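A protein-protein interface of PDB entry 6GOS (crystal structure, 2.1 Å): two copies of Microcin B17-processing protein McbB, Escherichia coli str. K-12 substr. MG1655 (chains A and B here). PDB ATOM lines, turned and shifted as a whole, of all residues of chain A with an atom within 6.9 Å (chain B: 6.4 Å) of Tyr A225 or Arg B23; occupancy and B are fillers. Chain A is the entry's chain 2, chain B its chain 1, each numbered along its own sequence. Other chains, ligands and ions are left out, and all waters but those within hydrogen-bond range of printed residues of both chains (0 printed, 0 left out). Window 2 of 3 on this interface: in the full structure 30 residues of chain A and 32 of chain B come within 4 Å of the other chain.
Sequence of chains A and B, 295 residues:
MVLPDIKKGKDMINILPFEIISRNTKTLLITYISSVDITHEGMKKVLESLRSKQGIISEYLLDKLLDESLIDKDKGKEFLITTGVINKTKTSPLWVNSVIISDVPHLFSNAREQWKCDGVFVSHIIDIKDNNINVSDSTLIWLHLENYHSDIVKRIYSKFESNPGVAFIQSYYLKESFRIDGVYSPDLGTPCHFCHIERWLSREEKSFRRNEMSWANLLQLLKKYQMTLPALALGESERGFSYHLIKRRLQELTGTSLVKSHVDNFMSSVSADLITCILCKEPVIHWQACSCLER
Of the 9 printed residues of chain A, 6 touch a printed residue of chain B. Hydrophobic or aromatic side chains of chain A that line the printed part of chain B: Leu A221, Leu A222, Tyr A225 and Met A227. Along chain A the printed residues that touch a printed residue of chain B span positions 221 to 228. Printed residues of chain B that touch a printed residue of chain A: Ile B21, Ser B22, Arg B23, Lys B26, Leu B28 and Asp B37. Hydrophobic or aromatic side chains of chain B that line the printed part of chain A: Ile B21 and Leu B28. Among the printed residues, 11 pairs touch across the chains. Among the printed residues, no Asp or Glu carboxylate lies within 4 Å of a Lys or Arg side-chain nitrogen of the other chain.
The side-chain hydroxyl (OH) of Tyr A225 lies within hydrogen-bond range of the side-chain carboxylate (OD2) of Asp B37, at 3.1 Å. NE of Arg B23 sits close to O of Gln A226 (3.5 Å).
Among the printed residues, merely in contact across the chains: Tyr A225 with Lys B26 (3.0 Å), Leu A222 with Leu B28 (3.4 Å), Met A227 with Ile B21 (3.4 Å), Leu A221 with Leu B28 (3.6 Å), Tyr A225 with Arg B23 (3.7 Å), Thr A228 with Ile B21 (3.7 Å), Met A227 with Arg B23 (3.8 Å), Leu A222 with Ile B21 (3.95 Å) and Met A227 with Ser B22 (3.96 Å).
No position is printed for both chains. Of the 11 pairs that touch across the chains among the printed residues, none has its exchanged pair printed and touching as well.
Lys A223 touches none of the printed residues of chain B. Of chain B, only Arg B23, Lys B26 and Asp B37 come within 4 Å of Tyr A225. Of the printed residues of chain A, Ile B21 touches Leu A222, Met A227 and Thr A228. Of chain A, only Tyr A225, Gln A226 and Met A227 come within 4 Å of Arg B23. Printed residues of chain A within 4 Å of Lys B26: Tyr A225. Of the printed residues of chain A, Leu B28 touches Leu A221 (3.6 Å) and Leu A222 (3.4 Å). The nearest residue of chain B that does not touch Tyr A225 is Leu B28 (4.5 Å). The nearest printed residue of chain A that does not touch Ser B22 is Tyr A225 (7.3 Å).
The side-chain hydroxyl (OG1) of Thr B27 sits close to the side-chain hydroxyl (OG) of Ser B22 (3.5 Å). The backbone NH of Leu B28 sits at hydrogen-bond distance from the backbone carbonyl oxygen of Ile B21 (2.9 Å). The backbone NH (N) of Met A227 is in hydrogen-bond range of the backbone carbonyl oxygen (O) of Leu A222 (2.9 Å).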
ATOM      1  N   GLN A 220       4.151  -3.007  -0.821  1.00  0.00           N
ATOM      2  CA  GLN A 220       5.319  -3.892  -0.696  1.00  0.00           C
ATOM      3  C   GLN A 220       5.290  -4.980  -1.792  1.00  0.00           C
ATOM      4  O   GLN A 220       6.334  -5.310  -2.355  1.00  0.00           O
ATOM      5  CB  GLN A 220       5.467  -4.515   0.724  1.00  0.00           C
ATOM      6  CG  GLN A 220       5.562  -3.569   1.958  1.00  0.00           C
ATOM      7  CD  GLN A 220       6.723  -2.537   2.017  1.00  0.00           C
ATOM      8  OE1 GLN A 220       7.325  -2.158   1.009  1.00  0.00           O
ATOM      9  NE2 GLN A 220       6.994  -2.044   3.231  1.00  0.00           N
ATOM     10  N   LEU A 221       4.110  -5.514  -2.117  1.00  0.00           N
ATOM     11  CA  LEU A 221       4.002  -6.490  -3.197  1.00  0.00           C
ATOM     12  C   LEU A 221       4.304  -5.892  -4.585  1.00  0.00           C
ATOM     13  O   LEU A 221       4.833  -6.593  -5.422  1.00  0.00           O
ATOM     14  CB  LEU A 221       2.624  -7.166  -3.206  1.00  0.00           C
ATOM     15  CG  LEU A 221       2.525  -8.421  -4.080  1.00  0.00           C
ATOM     16  CD1 LEU A 221       3.243  -9.613  -3.438  1.00  0.00           C
ATOM     17  CD2 LEU A 221       1.077  -8.772  -4.368  1.00  0.00           C
ATOM     18  N   LEU A 222       3.951  -4.621  -4.828  1.00  0.00           N
ATOM     19  CA  LEU A 222       4.355  -3.932  -6.058  1.00  0.00           C
ATOM     20  C   LEU A 222       5.880  -3.753  -6.130  1.00  0.00           C
ATOM     21  O   LEU A 222       6.438  -3.861  -7.210  1.00  0.00           O
ATOM     22  CB  LEU A 222       3.674  -2.557  -6.205  1.00  0.00           C
ATOM     23  CG  LEU A 222       2.155  -2.540  -6.376  1.00  0.00           C
ATOM     24  CD1 LEU A 222       1.598  -1.138  -6.149  1.00  0.00           C
ATOM     25  CD2 LEU A 222       1.763  -3.042  -7.741  1.00  0.00           C
ATOM     26  N   LYS A 223       6.541  -3.450  -5.003  1.00  0.00           N
ATOM     27  CA  LYS A 223       8.020  -3.488  -4.949  1.00  0.00           C
ATOM     28  C   LYS A 223       8.536  -4.888  -5.358  1.00  0.00           C
ATOM     29  O   LYS A 223       9.249  -5.012  -6.360  1.00  0.00           O
ATOM     30  CB  LYS A 223       8.560  -3.070  -3.578  1.00  0.00           C
ATOM     31  N   LYS A 224       8.106  -5.938  -4.650  1.00  0.00           N
ATOM     32  CA  LYS A 224       8.576  -7.310  -4.901  1.00  0.00           C
ATOM     33  C   LYS A 224       8.377  -7.745  -6.357  1.00  0.00           C
ATOM     34  O   LYS A 224       9.236  -8.401  -6.934  1.00  0.00           O
ATOM     35  CB  LYS A 224       7.892  -8.315  -3.963  1.00  0.00           C
ATOM     36  N   TYR A 225       7.254  -7.354  -6.942  1.00  0.00           N
ATOM     37  CA  TYR A 225       6.908  -7.678  -8.329  1.00  0.00           C
ATOM     38  C   TYR A 225       7.421  -6.661  -9.372  1.00  0.00           C
ATOM     39  O   TYR A 225       7.174  -6.841 -10.565  1.00  0.00           O
ATOM     40  CB  TYR A 225       5.383  -7.795  -8.454  1.00  0.00           C
ATOM     41  CG  TYR A 225       4.725  -9.038  -7.863  1.00  0.00           C
ATOM     42  CD1 TYR A 225       5.408  -9.946  -7.020  1.00  0.00           C
ATOM     43  CD2 TYR A 225       3.375  -9.283  -8.130  1.00  0.00           C
ATOM     44  CE1 TYR A 225       4.754 -11.064  -6.500  1.00  0.00           C
ATOM     45  CE2 TYR A 225       2.720 -10.394  -7.622  1.00  0.00           C
ATOM     46  CZ  TYR A 225       3.400 -11.278  -6.814  1.00  0.00           C
ATOM     47  OH  TYR A 225       2.687 -12.353  -6.344  1.00  0.00           O
ATOM     48  N   GLN A 226       8.119  -5.606  -8.937  1.00  0.00           N
ATOM     49  CA  GLN A 226       8.696  -4.589  -9.831  1.00  0.00           C
ATOM     50  C   GLN A 226       7.643  -3.885 -10.705  1.00  0.00           C
ATOM     51  O   GLN A 226       7.821  -3.700 -11.913  1.00  0.00           O
ATOM     52  CB  GLN A 226       9.850  -5.203 -10.657  1.00  0.00           C
ATOM     53  CG  GLN A 226      11.061  -5.497  -9.774  1.00  0.00           C
ATOM     54  CD  GLN A 226      12.154  -6.313 -10.453  1.00  0.00           C
ATOM     55  OE1 GLN A 226      11.886  -7.196 -11.265  1.00  0.00           O
ATOM     56  NE2 GLN A 226      13.400  -6.030 -10.094  1.00  0.00           N
ATOM     57  N   MET A 227       6.531  -3.519 -10.072  1.00  0.00           N
ATOM     58  CA  MET A 227       5.425  -2.813 -10.732  1.00  0.00           C
ATOM     59  C   MET A 227       5.198  -1.425 -10.120  1.00  0.00           C
ATOM     60  O   MET A 227       5.447  -1.188  -8.927  1.00  0.00           O
ATOM     61  CB  MET A 227       4.139  -3.625 -10.619  1.00  0.00           C
ATOM     62  CG  MET A 227       4.223  -4.991 -11.272  1.00  0.00           C
ATOM     63  SD  MET A 227       2.961  -6.120 -10.660  1.00  0.00           S
ATOM     64  CE  MET A 227       1.600  -5.624 -11.675  1.00  0.00           C
ATOM     65  N   THR A 228       4.727  -0.515 -10.946  1.00  0.00           N
ATOM     66  CA  THR A 228       4.266   0.786 -10.473  1.00  0.00           C
ATOM     67  C   THR A 228       2.838   0.713  -9.887  1.00  0.00           C
ATOM     68  O   THR A 228       2.064  -0.208 -10.171  1.00  0.00           O
ATOM     69  CB  THR A 228       4.319   1.823 -11.595  1.00  0.00           C
ATOM     70  OG1 THR A 228       3.593   1.338 -12.724  1.00  0.00           O
ATOM     71  CG2 THR A 228       5.761   2.107 -11.995  1.00  0.00           C
ATOM     72  N   ILE B  21      -3.570  -4.735 -13.458  1.00  0.00           N
ATOM     73  CA  ILE B  21      -2.217  -4.608 -14.035  1.00  0.00           C
ATOM     74  C   ILE B  21      -1.473  -5.930 -13.982  1.00  0.00           C
ATOM     75  O   ILE B  21      -1.698  -6.715 -13.081  1.00  0.00           O
ATOM     76  CB  ILE B  21      -1.377  -3.530 -13.318  1.00  0.00           C
ATOM     77  CG1 ILE B  21      -1.377  -3.739 -11.801  1.00  0.00           C
ATOM     78  CG2 ILE B  21      -1.920  -2.138 -13.634  1.00  0.00           C
ATOM     79  CD1 ILE B  21      -0.383  -2.879 -11.055  1.00  0.00           C
ATOM     80  N   SER B  22      -0.582  -6.150 -14.940  1.00  0.00           N
ATOM     81  CA  SER B  22       0.207  -7.383 -15.009  1.00  0.00           C
ATOM     82  C   SER B  22       1.648  -7.099 -15.394  1.00  0.00           C
ATOM     83  O   SER B  22       1.927  -6.165 -16.139  1.00  0.00           O
ATOM     84  CB  SER B  22      -0.383  -8.353 -16.036  1.00  0.00           C
ATOM     85  OG  SER B  22      -1.784  -8.456 -15.929  1.00  0.00           O
ATOM     86  N   ARG B  23       2.552  -7.917 -14.874  1.00  0.00           N
ATOM     87  CA  ARG B  23       3.962  -7.917 -15.266  1.00  0.00           C
ATOM     88  C   ARG B  23       4.527  -9.286 -14.941  1.00  0.00           C
ATOM     89  O   ARG B  23       4.388  -9.757 -13.809  1.00  0.00           O
ATOM     90  CB  ARG B  23       4.748  -6.844 -14.516  1.00  0.00           C
ATOM     91  CG  ARG B  23       6.166  -6.663 -15.044  1.00  0.00           C
ATOM     92  CD  ARG B  23       7.043  -5.818 -14.127  1.00  0.00           C
ATOM     93  NE  ARG B  23       8.457  -6.120 -14.352  1.00  0.00           N
ATOM     94  CZ  ARG B  23       9.174  -5.728 -15.408  1.00  0.00           C
ATOM     95  NH1 ARG B  23       8.637  -4.977 -16.376  1.00  0.00           N
ATOM     96  NH2 ARG B  23      10.453  -6.090 -15.497  1.00  0.00           N
ATOM     97  N   ASN B  24       5.167  -9.921 -15.928  1.00  0.00           N
ATOM     98  CA  ASN B  24       5.569 -11.338 -15.831  1.00  0.00           C
ATOM     99  C   ASN B  24       4.297 -12.166 -15.517  1.00  0.00           C
ATOM    100  O   ASN B  24       3.258 -11.945 -16.168  1.00  0.00           O
ATOM    101  CB  ASN B  24       6.715 -11.537 -14.814  1.00  0.00           C
ATOM    102  N   THR B  25       4.344 -13.065 -14.524  1.00  0.00           N
ATOM    103  CA  THR B  25       3.179 -13.907 -14.200  1.00  0.00           C
ATOM    104  C   THR B  25       2.266 -13.316 -13.103  1.00  0.00           C
ATOM    105  O   THR B  25       1.353 -13.991 -12.628  1.00  0.00           O
ATOM    106  CB  THR B  25       3.611 -15.331 -13.785  1.00  0.00           C
ATOM    107  OG1 THR B  25       4.253 -15.273 -12.507  1.00  0.00           O
ATOM    108  CG2 THR B  25       4.553 -15.967 -14.835  1.00  0.00           C
ATOM    109  N   LYS B  26       2.482 -12.056 -12.731  1.00  0.00           N
ATOM    110  CA  LYS B  26       1.774 -11.440 -11.624  1.00  0.00           C
ATOM    111  C   LYS B  26       0.700 -10.477 -12.147  1.00  0.00           C
ATOM    112  O   LYS B  26       0.963  -9.669 -13.033  1.00  0.00           O
ATOM    113  CB  LYS B  26       2.784 -10.706 -10.762  1.00  0.00           C
ATOM    114  N   THR B  27      -0.512 -10.578 -11.595  1.00  0.00           N
ATOM    115  CA  THR B  27      -1.650  -9.734 -11.974  1.00  0.00           C
ATOM    116  C   THR B  27      -2.303  -9.230 -10.692  1.00  0.00           C
ATOM    117  O   THR B  27      -2.615 -10.033  -9.794  1.00  0.00           O
ATOM    118  CB  THR B  27      -2.686 -10.519 -12.811  1.00  0.00           C
ATOM    119  OG1 THR B  27      -2.012 -11.217 -13.859  1.00  0.00           O
ATOM    120  CG2 THR B  27      -3.709  -9.602 -13.440  1.00  0.00           C
ATOM    121  N   LEU B  28      -2.486  -7.908 -10.600  1.00  0.00           N
ATOM    122  CA  LEU B  28      -3.130  -7.296  -9.433  1.00  0.00           C
ATOM    123  C   LEU B  28      -4.324  -6.433  -9.831  1.00  0.00           C
ATOM    124  O   LEU B  28      -4.231  -5.637 -10.779  1.00  0.00           O
ATOM    125  CB  LEU B  28      -2.144  -6.432  -8.658  1.00  0.00           C
ATOM    126  CG  LEU B  28      -0.838  -7.086  -8.249  1.00  0.00           C
ATOM    127  CD1 LEU B  28       0.155  -6.064  -7.732  1.00  0.00           C
ATOM    128  CD2 LEU B  28      -1.114  -8.155  -7.217  1.00  0.00           C
ATOM    129  N   ASP B  37      -4.469 -10.066  -5.343  1.00  0.00           N
ATOM    130  CA  ASP B  37      -3.522 -10.803  -6.188  1.00  0.00           C
ATOM    131  C   ASP B  37      -4.349 -11.833  -6.973  1.00  0.00           C
ATOM    132  O   ASP B  37      -4.832 -12.787  -6.388  1.00  0.00           O
ATOM    133  CB  ASP B  37      -2.451 -11.488  -5.325  1.00  0.00           C
ATOM    134  CG  ASP B  37      -1.231 -11.941  -6.122  1.00  0.00           C
ATOM    135  OD1 ASP B  37      -1.208 -11.775  -7.363  1.00  0.00           O
ATOM    136  OD2 ASP B  37      -0.277 -12.471  -5.497  1.00  0.00           O
